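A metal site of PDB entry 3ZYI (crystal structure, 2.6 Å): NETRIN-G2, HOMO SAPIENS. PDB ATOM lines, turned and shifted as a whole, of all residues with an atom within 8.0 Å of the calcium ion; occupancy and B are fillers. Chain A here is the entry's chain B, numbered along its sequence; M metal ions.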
ATOM      1  N   LYS A  47     -13.190 -16.013  -9.623  1.00  0.00           N
ATOM      2  CA  LYS A  47     -14.182 -15.870 -10.702  1.00  0.00           C
ATOM      3  C   LYS A  47     -15.553 -15.353 -10.203  1.00  0.00           C
ATOM      4  O   LYS A  47     -16.315 -14.803 -10.992  1.00  0.00           O
ATOM      5  CB  LYS A  47     -14.329 -17.180 -11.509  1.00  0.00           C
ATOM      6  CG  LYS A  47     -14.907 -18.362 -10.735  1.00  0.00           C
ATOM      7  CD  LYS A  47     -15.131 -19.579 -11.616  1.00  0.00           C
ATOM      8  CE  LYS A  47     -15.986 -20.609 -10.926  1.00  0.00           C
ATOM      9  NZ  LYS A  47     -16.047 -21.883 -11.689  1.00  0.00           N
ATOM     10  N   PRO A  91     -23.715 -15.466 -23.395  1.00  0.00           N
ATOM     11  CA  PRO A  91     -23.029 -14.224 -22.985  1.00  0.00           C
ATOM     12  C   PRO A  91     -21.685 -14.450 -22.268  1.00  0.00           C
ATOM     13  O   PRO A  91     -21.465 -15.551 -21.770  1.00  0.00           O
ATOM     14  CB  PRO A  91     -24.067 -13.539 -22.090  1.00  0.00           C
ATOM     15  CG  PRO A  91     -24.824 -14.653 -21.482  1.00  0.00           C
ATOM     16  CD  PRO A  91     -24.861 -15.749 -22.508  1.00  0.00           C
ATOM     17  N   PRO A  92     -20.803 -13.412 -22.178  1.00  0.00           N
ATOM     18  CA  PRO A  92     -19.496 -13.602 -21.493  1.00  0.00           C
ATOM     19  C   PRO A  92     -19.534 -14.063 -20.043  1.00  0.00           C
ATOM     20  O   PRO A  92     -18.589 -14.724 -19.605  1.00  0.00           O
ATOM     21  CB  PRO A  92     -18.853 -12.222 -21.604  1.00  0.00           C
ATOM     22  CG  PRO A  92     -19.485 -11.590 -22.779  1.00  0.00           C
ATOM     23  CD  PRO A  92     -20.909 -12.051 -22.739  1.00  0.00           C
ATOM     24  N   ARG A  93     -20.605 -13.746 -19.299  1.00  0.00           N
ATOM     25  CA  ARG A  93     -20.808 -14.116 -17.891  1.00  0.00           C
ATOM     26  C   ARG A  93     -20.752 -15.623 -17.618  1.00  0.00           C
ATOM     27  O   ARG A  93     -20.396 -16.031 -16.511  1.00  0.00           O
ATOM     28  CB  ARG A  93     -22.112 -13.497 -17.342  1.00  0.00           C
ATOM     29  CG  ARG A  93     -23.394 -13.974 -18.025  1.00  0.00           C
ATOM     30  CD  ARG A  93     -24.635 -13.345 -17.421  1.00  0.00           C
ATOM     31  NE  ARG A  93     -25.864 -14.006 -17.889  1.00  0.00           N
ATOM     32  CZ  ARG A  93     -26.452 -15.019 -17.261  1.00  0.00           C
ATOM     33  NH1 ARG A  93     -25.959 -15.493 -16.128  1.00  0.00           N
ATOM     34  NH2 ARG A  93     -27.564 -15.551 -17.759  1.00  0.00           N
ATOM     35  N   LEU A  94     -21.082 -16.459 -18.639  1.00  0.00           N
ATOM     36  CA  LEU A  94     -21.090 -17.922 -18.571  1.00  0.00           C
ATOM     37  C   LEU A  94     -19.719 -18.572 -18.357  1.00  0.00           C
ATOM     38  O   LEU A  94     -19.649 -19.765 -18.056  1.00  0.00           O
ATOM     39  CB  LEU A  94     -21.833 -18.545 -19.775  1.00  0.00           C
ATOM     40  CG  LEU A  94     -23.317 -18.198 -19.966  1.00  0.00           C
ATOM     41  CD1 LEU A  94     -23.932 -19.044 -21.067  1.00  0.00           C
ATOM     42  CD2 LEU A  94     -24.126 -18.407 -18.682  1.00  0.00           C
ATOM     43  N   MET A  95     -18.631 -17.776 -18.465  1.00  0.00           N
ATOM     44  CA  MET A  95     -17.249 -18.214 -18.252  1.00  0.00           C
ATOM     45  C   MET A  95     -16.876 -18.262 -16.758  1.00  0.00           C
ATOM     46  O   MET A  95     -15.819 -18.786 -16.416  1.00  0.00           O
ATOM     47  CB  MET A  95     -16.270 -17.291 -18.994  1.00  0.00           C
ATOM     48  CG  MET A  95     -16.328 -17.415 -20.488  1.00  0.00           C
ATOM     49  SD  MET A  95     -15.064 -16.460 -21.362  1.00  0.00           S
ATOM     50  CE  MET A  95     -15.856 -14.877 -21.468  1.00  0.00           C
ATOM     51  N   PHE A  96     -17.741 -17.693 -15.875  1.00  0.00           N
ATOM     52  CA  PHE A  96     -17.441 -17.597 -14.430  1.00  0.00           C
ATOM     53  C   PHE A  96     -18.500 -18.129 -13.476  1.00  0.00           C
ATOM     54  O   PHE A  96     -18.200 -18.309 -12.290  1.00  0.00           O
ATOM     55  CB  PHE A  96     -17.054 -16.147 -14.063  1.00  0.00           C
ATOM     56  CG  PHE A  96     -16.348 -15.391 -15.167  1.00  0.00           C
ATOM     57  CD1 PHE A  96     -15.010 -15.629 -15.457  1.00  0.00           C
ATOM     58  CD2 PHE A  96     -17.037 -14.489 -15.963  1.00  0.00           C
ATOM     59  CE1 PHE A  96     -14.363 -14.971 -16.507  1.00  0.00           C
ATOM     60  CE2 PHE A  96     -16.397 -13.820 -17.009  1.00  0.00           C
ATOM     61  CZ  PHE A  96     -15.066 -14.065 -17.271  1.00  0.00           C
ATOM     62  N   ASP A  97     -19.734 -18.382 -13.957  1.00  0.00           N
ATOM     63  CA  ASP A  97     -20.846 -18.879 -13.132  1.00  0.00           C
ATOM     64  C   ASP A  97     -20.612 -20.263 -12.535  1.00  0.00           C
ATOM     65  O   ASP A  97     -19.861 -21.062 -13.090  1.00  0.00           O
ATOM     66  CB  ASP A  97     -22.186 -18.798 -13.887  1.00  0.00           C
ATOM     67  CG  ASP A  97     -22.367 -19.701 -15.104  1.00  0.00           C
ATOM     68  OD1 ASP A  97     -21.357 -20.271 -15.580  1.00  0.00           O
ATOM     69  OD2 ASP A  97     -23.514 -19.809 -15.593  1.00  0.00           O
ATOM     70  N   LYS A  98     -21.250 -20.541 -11.377  1.00  0.00           N
ATOM     71  CA  LYS A  98     -21.183 -21.828 -10.678  1.00  0.00           C
ATOM     72  C   LYS A  98     -21.976 -22.852 -11.490  1.00  0.00           C
ATOM     73  O   LYS A  98     -23.095 -22.545 -11.928  1.00  0.00           O
ATOM     74  CB  LYS A  98     -21.727 -21.704  -9.251  1.00  0.00           C
ATOM     75  N   GLU A  99     -21.391 -24.034 -11.743  1.00  0.00           N
ATOM     76  CA  GLU A  99     -22.026 -25.059 -12.572  1.00  0.00           C
ATOM     77  C   GLU A  99     -22.451 -26.323 -11.854  1.00  0.00           C
ATOM     78  O   GLU A  99     -21.711 -26.836 -11.000  1.00  0.00           O
ATOM     79  CB  GLU A  99     -21.150 -25.411 -13.789  1.00  0.00           C
ATOM     80  CG  GLU A  99     -21.022 -24.286 -14.804  1.00  0.00           C
ATOM     81  CD  GLU A  99     -20.074 -24.537 -15.964  1.00  0.00           C
ATOM     82  OE1 GLU A  99     -19.142 -25.351 -15.827  1.00  0.00           O
ATOM     83  OE2 GLU A  99     -20.258 -23.863 -17.006  1.00  0.00           O
ATOM     84  N   LEU A 103     -23.916 -29.906 -16.435  1.00  0.00           N
ATOM     85  CA  LEU A 103     -24.669 -28.800 -17.044  1.00  0.00           C
ATOM     86  C   LEU A 103     -23.776 -27.574 -17.278  1.00  0.00           C
ATOM     87  O   LEU A 103     -23.942 -26.527 -16.638  1.00  0.00           O
ATOM     88  CB  LEU A 103     -25.907 -28.456 -16.191  1.00  0.00           C
ATOM     89  CG  LEU A 103     -27.027 -29.496 -16.200  1.00  0.00           C
ATOM     90  CD1 LEU A 103     -27.587 -29.707 -14.813  1.00  0.00           C
ATOM     91  CD2 LEU A 103     -28.107 -29.118 -17.193  1.00  0.00           C
ATOM     92  N   ALA A 104     -22.817 -27.726 -18.212  1.00  0.00           N
ATOM     93  CA  ALA A 104     -21.850 -26.682 -18.568  1.00  0.00           C
ATOM     94  C   ALA A 104     -22.473 -25.537 -19.363  1.00  0.00           C
ATOM     95  O   ALA A 104     -23.213 -25.763 -20.324  1.00  0.00           O
ATOM     96  CB  ALA A 104     -20.685 -27.284 -19.335  1.00  0.00           C
ATOM     97  N   THR A 105     -22.165 -24.294 -18.938  1.00  0.00           N
ATOM     98  CA  THR A 105     -22.616 -23.043 -19.561  1.00  0.00           C
ATOM     99  C   THR A 105     -21.379 -22.366 -20.143  1.00  0.00           C
ATOM    100  O   THR A 105     -20.379 -22.253 -19.452  1.00  0.00           O
ATOM    101  CB  THR A 105     -23.329 -22.150 -18.536  1.00  0.00           C
ATOM    102  OG1 THR A 105     -22.492 -21.975 -17.392  1.00  0.00           O
ATOM    103  CG2 THR A 105     -24.697 -22.696 -18.123  1.00  0.00           C
ATOM    104  N   TYR A 106     -21.447 -21.938 -21.409  1.00  0.00           N
ATOM    105  CA  TYR A 106     -20.289 -21.362 -22.079  1.00  0.00           C
ATOM    106  C   TYR A 106     -20.538 -20.074 -22.852  1.00  0.00           C
ATOM    107  O   TYR A 106     -21.620 -19.891 -23.395  1.00  0.00           O
ATOM    108  CB  TYR A 106     -19.631 -22.404 -23.009  1.00  0.00           C
ATOM    109  CG  TYR A 106     -20.521 -22.913 -24.122  1.00  0.00           C
ATOM    110  CD1 TYR A 106     -21.349 -24.011 -23.943  1.00  0.00           C
ATOM    111  CD2 TYR A 106     -20.499 -22.308 -25.384  1.00  0.00           C
ATOM    112  CE1 TYR A 106     -22.175 -24.478 -24.974  1.00  0.00           C
ATOM    113  CE2 TYR A 106     -21.309 -22.779 -26.426  1.00  0.00           C
ATOM    114  CZ  TYR A 106     -22.147 -23.853 -26.215  1.00  0.00           C
ATOM    115  OH  TYR A 106     -22.948 -24.314 -27.226  1.00  0.00           O
ATOM    116  N   TRP A 107     -19.506 -19.216 -22.955  1.00  0.00           N
ATOM    117  CA  TRP A 107     -19.535 -18.024 -23.805  1.00  0.00           C
ATOM    118  C   TRP A 107     -19.089 -18.523 -25.164  1.00  0.00           C
ATOM    119  O   TRP A 107     -18.139 -19.298 -25.237  1.00  0.00           O
ATOM    120  CB  TRP A 107     -18.566 -16.934 -23.302  1.00  0.00           C
ATOM    121  CG  TRP A 107     -18.198 -15.929 -24.373  1.00  0.00           C
ATOM    122  CD1 TRP A 107     -18.943 -14.856 -24.775  1.00  0.00           C
ATOM    123  CD2 TRP A 107     -17.057 -15.969 -25.235  1.00  0.00           C
ATOM    124  NE1 TRP A 107     -18.303 -14.196 -25.798  1.00  0.00           N
ATOM    125  CE2 TRP A 107     -17.146 -14.858 -26.112  1.00  0.00           C
ATOM    126  CE3 TRP A 107     -15.942 -16.829 -25.361  1.00  0.00           C
ATOM    127  CZ2 TRP A 107     -16.174 -14.576 -27.079  1.00  0.00           C
ATOM    128  CZ3 TRP A 107     -14.996 -16.562 -26.324  1.00  0.00           C
ATOM    129  CH2 TRP A 107     -15.107 -15.445 -27.163  1.00  0.00           C
ATOM    130  N   THR A 140     -11.263 -23.647 -19.471  1.00  0.00           N
ATOM    131  CA  THR A 140     -11.985 -24.806 -20.018  1.00  0.00           C
ATOM    132  C   THR A 140     -12.702 -24.408 -21.301  1.00  0.00           C
ATOM    133  O   THR A 140     -13.646 -23.626 -21.278  1.00  0.00           O
ATOM    134  CB  THR A 140     -12.930 -25.417 -18.976  1.00  0.00           C
ATOM    135  OG1 THR A 140     -12.225 -25.632 -17.755  1.00  0.00           O
ATOM    136  CG2 THR A 140     -13.581 -26.719 -19.460  1.00  0.00           C
ATOM    137  N   GLU A 142     -14.831 -25.418 -24.897  1.00  0.00           N
ATOM    138  CA  GLU A 142     -15.834 -26.349 -25.412  1.00  0.00           C
ATOM    139  C   GLU A 142     -15.668 -26.465 -26.919  1.00  0.00           C
ATOM    140  O   GLU A 142     -15.522 -25.452 -27.609  1.00  0.00           O
ATOM    141  CB  GLU A 142     -17.276 -25.896 -25.074  1.00  0.00           C
ATOM    142  CG  GLU A 142     -17.614 -25.942 -23.590  1.00  0.00           C
ATOM    143  CD  GLU A 142     -17.465 -27.276 -22.899  1.00  0.00           C
ATOM    144  OE1 GLU A 142     -17.981 -28.290 -23.423  1.00  0.00           O
ATOM    145  OE2 GLU A 142     -16.846 -27.317 -21.812  1.00  0.00           O
ATOM    146  N   ILE A 278     -15.895 -20.921 -24.313  1.00  0.00           N
ATOM    147  CA  ILE A 278     -15.269 -21.097 -23.002  1.00  0.00           C
ATOM    148  C   ILE A 278     -16.332 -21.317 -21.937  1.00  0.00           C
ATOM    149  O   ILE A 278     -17.142 -20.428 -21.670  1.00  0.00           O
ATOM    150  CB  ILE A 278     -14.300 -19.931 -22.636  1.00  0.00           C
ATOM    151  CG1 ILE A 278     -13.368 -19.568 -23.821  1.00  0.00           C
ATOM    152  CG2 ILE A 278     -13.490 -20.257 -21.384  1.00  0.00           C
ATOM    153  CD1 ILE A 278     -12.801 -18.159 -23.833  1.00  0.00           C
ATOM    154  N   SER A 279     -16.339 -22.512 -21.326  1.00  0.00           N
ATOM    155  CA  SER A 279     -17.293 -22.866 -20.270  1.00  0.00           C
ATOM    156  C   SER A 279     -16.867 -22.369 -18.897  1.00  0.00           C
ATOM    157  O   SER A 279     -17.731 -22.068 -18.072  1.00  0.00           O
ATOM    158  CB  SER A 279     -17.561 -24.363 -20.253  1.00  0.00           C
ATOM    159  OG  SER A 279     -16.365 -25.114 -20.089  1.00  0.00           O
ATOM    160  N   ASN A 280     -15.558 -22.303 -18.645  1.00  0.00           N
ATOM    161  CA  ASN A 280     -15.046 -21.866 -17.344  1.00  0.00           C
ATOM    162  C   ASN A 280     -13.613 -21.357 -17.386  1.00  0.00           C
ATOM    163  O   ASN A 280     -12.779 -21.894 -18.103  1.00  0.00           O
ATOM    164  CB  ASN A 280     -15.163 -22.992 -16.312  1.00  0.00           C
ATOM    165  CG  ASN A 280     -15.191 -22.499 -14.888  1.00  0.00           C
ATOM    166  OD1 ASN A 280     -16.116 -21.785 -14.479  1.00  0.00           O
ATOM    167  ND2 ASN A 280     -14.196 -22.880 -14.114  1.00  0.00           N
ATOM    168  N   ILE A 281     -13.345 -20.315 -16.583  1.00  0.00           N
ATOM    169  CA  ILE A 281     -12.022 -19.752 -16.348  1.00  0.00           C
ATOM    170  C   ILE A 281     -11.871 -19.778 -14.829  1.00  0.00           C
ATOM    171  O   ILE A 281     -12.451 -18.944 -14.119  1.00  0.00           O
ATOM    172  CB  ILE A 281     -11.781 -18.337 -16.972  1.00  0.00           C
ATOM    173  CG1 ILE A 281     -12.095 -18.321 -18.494  1.00  0.00           C
ATOM    174  CG2 ILE A 281     -10.332 -17.889 -16.708  1.00  0.00           C
ATOM    175  CD1 ILE A 281     -12.317 -16.960 -19.101  1.00  0.00           C
HETATM  176 CA    CA M   1     -19.756 -21.719 -17.049  1.00  0.00          CA
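The backbone carbonyl oxygen (O) of Thr 140 sits at hydrogen-bond distance from the backbone NH (N) of Ser 279 (2.9 Å). OG of Ser 279 lies within hydrogen-bond range of OE2 of Glu 142, at 2.8 Å.
The calcium ion is bound by O of Leu 94, OE2 of Glu 99, O of Ser 279, O of Thr 105, OD1 of Asp 97 and OG1 of Thr 105. The calcium ion has six donor atoms within binding distance.
Within 4 Å of the calcium ion: Leu 94, Asp 97, Glu 99, Thr 105 and Ser 279.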
